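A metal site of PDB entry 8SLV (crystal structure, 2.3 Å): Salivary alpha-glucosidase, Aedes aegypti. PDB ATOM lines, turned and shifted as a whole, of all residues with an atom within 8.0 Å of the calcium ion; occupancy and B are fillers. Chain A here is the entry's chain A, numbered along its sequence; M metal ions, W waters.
The calcium ion is bound by OD1 of Asp 39 (2.1 Å), O of Ile 43 (2.2 Å), OD2 of Asp 45 (2.2 Å), OD1 of Asp 37 (2.3 Å), water W1 (2.3 Å) and OD1 of Asp 41 (2.4 Å). The calcium ion has six donor atoms within binding distance.
OD1 of Asp 45 lies within hydrogen-bond range of OG of Ser 38, at 2.7 Å. The backbone NH of Asp 45 lies within hydrogen-bond range of the backbone carbonyl oxygen of Lys 36, 3.2 Å away. The backbone NH of Gly 48 is in hydrogen-bond range of the side-chain carboxylate of Asp 45. OD1 of Asp 45 sits close to N of Asp 47, 3.4 Å away. The backbone NH (N) of Gly 40 sits at hydrogen-bond distance from the side-chain carboxylate (OD2) of Asp 37 (3.4 Å). The side-chain carboxylate of Asp 37 lies within hydrogen-bond range of the backbone NH of Gly 42, 2.7 Å away. The side-chain carboxylate (OD2) of Asp 37 is in hydrogen-bond range of the side-chain hydroxyl (OG) of Ser 439. The backbone NH (N) of Asp 37 sits at hydrogen-bond distance from the backbone carbonyl oxygen (O) of Phe 438.
Water W1 bridges the side-chain carboxylate of Asp 41 (2.5 Å) and the backbone carbonyl oxygen of Glu 90 (2.5 Å).
Five residues have an atom within 4 Å of the calcium ion: Asp 37, Asp 39, Asp 41, Ile 43 and Asp 45. The nearest printed residue that does not touch the calcium ion is Ser 38 (4.1 Å).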
ATOM      1  N   PRO A  32      -0.851  -0.143 -14.568  1.00  0.00           N
ATOM      2  CA  PRO A  32      -1.441  -0.764 -13.355  1.00  0.00           C
ATOM      3  C   PRO A  32      -0.568  -1.811 -12.700  1.00  0.00           C
ATOM      4  O   PRO A  32      -0.573  -1.912 -11.466  1.00  0.00           O
ATOM      5  CB  PRO A  32      -2.738  -1.400 -13.891  1.00  0.00           C
ATOM      6  CG  PRO A  32      -3.035  -0.677 -15.163  1.00  0.00           C
ATOM      7  CD  PRO A  32      -1.727  -0.227 -15.740  1.00  0.00           C
ATOM      8  N   ARG A  33       0.189  -2.587 -13.475  1.00  0.00           N
ATOM      9  CA  ARG A  33       1.047  -3.588 -12.875  1.00  0.00           C
ATOM     10  C   ARG A  33       2.079  -2.986 -11.926  1.00  0.00           C
ATOM     11  O   ARG A  33       2.552  -3.672 -11.020  1.00  0.00           O
ATOM     12  CB  ARG A  33       1.753  -4.389 -13.961  1.00  0.00           C
ATOM     13  CG  ARG A  33       2.092  -5.788 -13.535  1.00  0.00           C
ATOM     14  CD  ARG A  33       2.559  -6.638 -14.716  1.00  0.00           C
ATOM     15  NE  ARG A  33       2.696  -8.032 -14.312  1.00  0.00           N
ATOM     16  CZ  ARG A  33       1.660  -8.872 -14.179  1.00  0.00           C
ATOM     17  NH1 ARG A  33       0.424  -8.469 -14.436  1.00  0.00           N
ATOM     18  NH2 ARG A  33       1.878 -10.111 -13.779  1.00  0.00           N
ATOM     19  N   LYS A  36       0.314   0.394  -7.729  1.00  0.00           N
ATOM     20  CA  LYS A  36       0.177   0.129  -6.306  1.00  0.00           C
ATOM     21  C   LYS A  36      -0.325  -1.300  -6.096  1.00  0.00           C
ATOM     22  O   LYS A  36      -1.415  -1.635  -6.568  1.00  0.00           O
ATOM     23  CB  LYS A  36      -0.757   1.144  -5.651  1.00  0.00           C
ATOM     24  CG  LYS A  36      -1.021   0.932  -4.163  1.00  0.00           C
ATOM     25  CD  LYS A  36       0.299   0.937  -3.369  1.00  0.00           C
ATOM     26  CE  LYS A  36       0.081   1.047  -1.862  1.00  0.00           C
ATOM     27  NZ  LYS A  36      -0.761  -0.078  -1.343  1.00  0.00           N
ATOM     28  N   ASP A  37       0.460  -2.120  -5.412  1.00  0.00           N
ATOM     29  CA  ASP A  37      -0.002  -3.439  -4.963  1.00  0.00           C
ATOM     30  C   ASP A  37      -0.877  -3.266  -3.731  1.00  0.00           C
ATOM     31  O   ASP A  37      -0.544  -2.519  -2.805  1.00  0.00           O
ATOM     32  CB  ASP A  37       1.205  -4.331  -4.664  1.00  0.00           C
ATOM     33  CG  ASP A  37       0.839  -5.793  -4.400  1.00  0.00           C
ATOM     34  OD1 ASP A  37      -0.311  -6.205  -4.651  1.00  0.00           O
ATOM     35  OD2 ASP A  37       1.718  -6.563  -3.959  1.00  0.00           O
ATOM     36  N   SER A  38      -2.028  -3.939  -3.711  1.00  0.00           N
ATOM     37  CA  SER A  38      -2.896  -3.893  -2.554  1.00  0.00           C
ATOM     38  C   SER A  38      -3.097  -5.234  -1.869  1.00  0.00           C
ATOM     39  O   SER A  38      -3.710  -5.282  -0.801  1.00  0.00           O
ATOM     40  CB  SER A  38      -4.277  -3.331  -2.929  1.00  0.00           C
ATOM     41  OG  SER A  38      -5.002  -4.294  -3.665  1.00  0.00           O
ATOM     42  N   ASP A  39      -2.610  -6.325  -2.448  1.00  0.00           N
ATOM     43  CA  ASP A  39      -2.920  -7.649  -1.916  1.00  0.00           C
ATOM     44  C   ASP A  39      -1.674  -8.522  -1.778  1.00  0.00           C
ATOM     45  O   ASP A  39      -1.795  -9.746  -1.731  1.00  0.00           O
ATOM     46  CB  ASP A  39      -3.978  -8.351  -2.779  1.00  0.00           C
ATOM     47  CG  ASP A  39      -3.592  -8.400  -4.261  1.00  0.00           C
ATOM     48  OD1 ASP A  39      -2.475  -7.976  -4.589  1.00  0.00           O
ATOM     49  OD2 ASP A  39      -4.405  -8.854  -5.102  1.00  0.00           O
ATOM     50  N   GLY A  40      -0.495  -7.916  -1.769  1.00  0.00           N
ATOM     51  CA  GLY A  40       0.718  -8.619  -1.373  1.00  0.00           C
ATOM     52  C   GLY A  40       1.246  -9.673  -2.338  1.00  0.00           C
ATOM     53  O   GLY A  40       2.028 -10.527  -1.926  1.00  0.00           O
ATOM     54  N   ASP A  41       0.856  -9.640  -3.611  1.00  0.00           N
ATOM     55  CA  ASP A  41       1.498 -10.540  -4.579  1.00  0.00           C
ATOM     56  C   ASP A  41       2.656  -9.884  -5.325  1.00  0.00           C
ATOM     57  O   ASP A  41       3.266 -10.525  -6.182  1.00  0.00           O
ATOM     58  CB  ASP A  41       0.455 -11.090  -5.567  1.00  0.00           C
ATOM     59  CG  ASP A  41      -0.253  -9.987  -6.353  1.00  0.00           C
ATOM     60  OD1 ASP A  41      -0.020  -8.787  -6.086  1.00  0.00           O
ATOM     61  OD2 ASP A  41      -1.052 -10.330  -7.257  1.00  0.00           O
ATOM     62  N   GLY A  42       3.016  -8.638  -4.986  1.00  0.00           N
ATOM     63  CA  GLY A  42       4.051  -7.945  -5.719  1.00  0.00           C
ATOM     64  C   GLY A  42       3.624  -7.400  -7.063  1.00  0.00           C
ATOM     65  O   GLY A  42       4.481  -6.962  -7.840  1.00  0.00           O
ATOM     66  N   ILE A  43       2.325  -7.396  -7.356  1.00  0.00           N
ATOM     67  CA  ILE A  43       1.785  -6.956  -8.641  1.00  0.00           C
ATOM     68  C   ILE A  43       0.787  -5.846  -8.377  1.00  0.00           C
ATOM     69  O   ILE A  43      -0.111  -5.997  -7.551  1.00  0.00           O
ATOM     70  CB  ILE A  43       1.104  -8.120  -9.389  1.00  0.00           C
ATOM     71  CG1 ILE A  43       2.123  -9.237  -9.647  1.00  0.00           C
ATOM     72  CG2 ILE A  43       0.473  -7.626 -10.686  1.00  0.00           C
ATOM     73  CD1 ILE A  43       1.507 -10.566 -10.056  1.00  0.00           C
ATOM     74  N   GLY A  44       0.929  -4.720  -9.087  1.00  0.00           N
ATOM     75  CA  GLY A  44      -0.059  -3.668  -8.972  1.00  0.00           C
ATOM     76  C   GLY A  44      -1.416  -4.144  -9.451  1.00  0.00           C
ATOM     77  O   GLY A  44      -1.525  -5.019 -10.318  1.00  0.00           O
ATOM     78  N   ASP A  45      -2.476  -3.565  -8.873  1.00  0.00           N
ATOM     79  CA  ASP A  45      -3.823  -4.053  -9.132  1.00  0.00           C
ATOM     80  C   ASP A  45      -4.822  -2.900  -9.071  1.00  0.00           C
ATOM     81  O   ASP A  45      -4.491  -1.777  -8.681  1.00  0.00           O
ATOM     82  CB  ASP A  45      -4.183  -5.138  -8.132  1.00  0.00           C
ATOM     83  CG  ASP A  45      -3.886  -4.715  -6.699  1.00  0.00           C
ATOM     84  OD1 ASP A  45      -4.503  -3.742  -6.212  1.00  0.00           O
ATOM     85  OD2 ASP A  45      -2.976  -5.313  -6.090  1.00  0.00           O
ATOM     86  N   LEU A  46      -6.067  -3.211  -9.455  1.00  0.00           N
ATOM     87  CA  LEU A  46      -7.116  -2.179  -9.538  1.00  0.00           C
ATOM     88  C   LEU A  46      -7.394  -1.540  -8.174  1.00  0.00           C
ATOM     89  O   LEU A  46      -7.545  -0.323  -8.067  1.00  0.00           O
ATOM     90  CB  LEU A  46      -8.407  -2.788 -10.117  1.00  0.00           C
ATOM     91  CG  LEU A  46      -8.409  -3.284 -11.567  1.00  0.00           C
ATOM     92  CD1 LEU A  46      -9.819  -3.482 -12.109  1.00  0.00           C
ATOM     93  CD2 LEU A  46      -7.609  -2.348 -12.487  1.00  0.00           C
ATOM     94  N   ASP A  47      -7.485  -2.348  -7.120  1.00  0.00           N
ATOM     95  CA  ASP A  47      -7.682  -1.783  -5.790  1.00  0.00           C
ATOM     96  C   ASP A  47      -6.551  -0.838  -5.420  1.00  0.00           C
ATOM     97  O   ASP A  47      -6.767   0.204  -4.787  1.00  0.00           O
ATOM     98  CB  ASP A  47      -7.819  -2.898  -4.737  1.00  0.00           C
ATOM     99  CG  ASP A  47      -9.215  -3.494  -4.667  1.00  0.00           C
ATOM    100  OD1 ASP A  47     -10.182  -2.908  -5.223  1.00  0.00           O
ATOM    101  OD2 ASP A  47      -9.343  -4.560  -4.030  1.00  0.00           O
ATOM    102  N   GLY A  48      -5.315  -1.195  -5.819  1.00  0.00           N
ATOM    103  CA  GLY A  48      -4.194  -0.301  -5.603  1.00  0.00           C
ATOM    104  C   GLY A  48      -4.361   1.027  -6.304  1.00  0.00           C
ATOM    105  O   GLY A  48      -4.100   2.092  -5.723  1.00  0.00           O
ATOM    106  N   THR A  89      -7.124 -11.582 -13.733  1.00  0.00           N
ATOM    107  CA  THR A  89      -7.358 -12.060 -12.373  1.00  0.00           C
ATOM    108  C   THR A  89      -6.561 -11.271 -11.334  1.00  0.00           C
ATOM    109  O   THR A  89      -7.137 -10.729 -10.378  1.00  0.00           O
ATOM    110  CB  THR A  89      -6.988 -13.545 -12.298  1.00  0.00           C
ATOM    111  OG1 THR A  89      -7.865 -14.292 -13.130  1.00  0.00           O
ATOM    112  CG2 THR A  89      -7.060 -14.052 -10.872  1.00  0.00           C
ATOM    113  N   GLU A  90      -5.235 -11.192 -11.483  1.00  0.00           N
ATOM    114  CA  GLU A  90      -4.462 -10.560 -10.417  1.00  0.00           C
ATOM    115  C   GLU A  90      -4.759  -9.063 -10.294  1.00  0.00           C
ATOM    116  O   GLU A  90      -4.521  -8.497  -9.230  1.00  0.00           O
ATOM    117  CB  GLU A  90      -2.958 -10.779 -10.599  1.00  0.00           C
ATOM    118  CG  GLU A  90      -2.335 -10.125 -11.819  1.00  0.00           C
ATOM    119  CD  GLU A  90      -2.246 -11.085 -12.992  1.00  0.00           C
ATOM    120  OE1 GLU A  90      -1.354 -10.913 -13.858  1.00  0.00           O
ATOM    121  OE2 GLU A  90      -3.094 -12.016 -13.019  1.00  0.00           O
ATOM    122  N   TYR A  91      -5.309  -8.422 -11.332  1.00  0.00           N
ATOM    123  CA  TYR A  91      -5.656  -7.009 -11.196  1.00  0.00           C
ATOM    124  C   TYR A  91      -6.968  -6.809 -10.443  1.00  0.00           C
ATOM    125  O   TYR A  91      -7.184  -5.738  -9.867  1.00  0.00           O
ATOM    126  CB  TYR A  91      -5.768  -6.362 -12.578  1.00  0.00           C
ATOM    127  CG  TYR A  91      -4.480  -6.288 -13.360  1.00  0.00           C
ATOM    128  CD1 TYR A  91      -3.237  -6.267 -12.719  1.00  0.00           C
ATOM    129  CD2 TYR A  91      -4.491  -6.249 -14.756  1.00  0.00           C
ATOM    130  CE1 TYR A  91      -2.046  -6.191 -13.459  1.00  0.00           C
ATOM    131  CE2 TYR A  91      -3.317  -6.197 -15.502  1.00  0.00           C
ATOM    132  CZ  TYR A  91      -2.104  -6.168 -14.845  1.00  0.00           C
ATOM    133  OH  TYR A  91      -0.940  -6.096 -15.598  1.00  0.00           O
ATOM    134  N   GLY A  92      -7.838  -7.825 -10.424  1.00  0.00           N
ATOM    135  CA  GLY A  92      -9.133  -7.705  -9.780  1.00  0.00           C
ATOM    136  C   GLY A  92     -10.227  -8.406 -10.541  1.00  0.00           C
ATOM    137  O   GLY A  92      -9.978  -9.357 -11.295  1.00  0.00           O
ATOM    138  N   PHE A 438       5.092   0.443  -2.464  1.00  0.00           N
ATOM    139  CA  PHE A 438       4.285  -0.105  -3.553  1.00  0.00           C
ATOM    140  C   PHE A 438       3.666  -1.443  -3.188  1.00  0.00           C
ATOM    141  O   PHE A 438       2.621  -1.810  -3.725  1.00  0.00           O
ATOM    142  CB  PHE A 438       5.166  -0.261  -4.800  1.00  0.00           C
ATOM    143  CG  PHE A 438       4.680  -1.304  -5.788  1.00  0.00           C
ATOM    144  CD1 PHE A 438       3.714  -0.990  -6.718  1.00  0.00           C
ATOM    145  CD2 PHE A 438       5.204  -2.584  -5.771  1.00  0.00           C
ATOM    146  CE1 PHE A 438       3.277  -1.924  -7.628  1.00  0.00           C
ATOM    147  CE2 PHE A 438       4.784  -3.544  -6.685  1.00  0.00           C
ATOM    148  CZ  PHE A 438       3.804  -3.214  -7.614  1.00  0.00           C
ATOM    149  N   SER A 439       4.311  -2.194  -2.299  1.00  0.00           N
ATOM    150  CA  SER A 439       3.872  -3.545  -2.006  1.00  0.00           C
ATOM    151  C   SER A 439       4.480  -3.978  -0.679  1.00  0.00           C
ATOM    152  O   SER A 439       5.599  -3.584  -0.332  1.00  0.00           O
ATOM    153  CB  SER A 439       4.293  -4.523  -3.098  1.00  0.00           C
ATOM    154  OG  SER A 439       3.878  -5.829  -2.752  1.00  0.00           O
HETATM  155 CA    CA M   1      -1.596  -7.050  -6.296  1.00  0.00          CA
HETATM  156  O   HOH W   1      -2.331  -8.334  -8.014  1.00  0.00           O
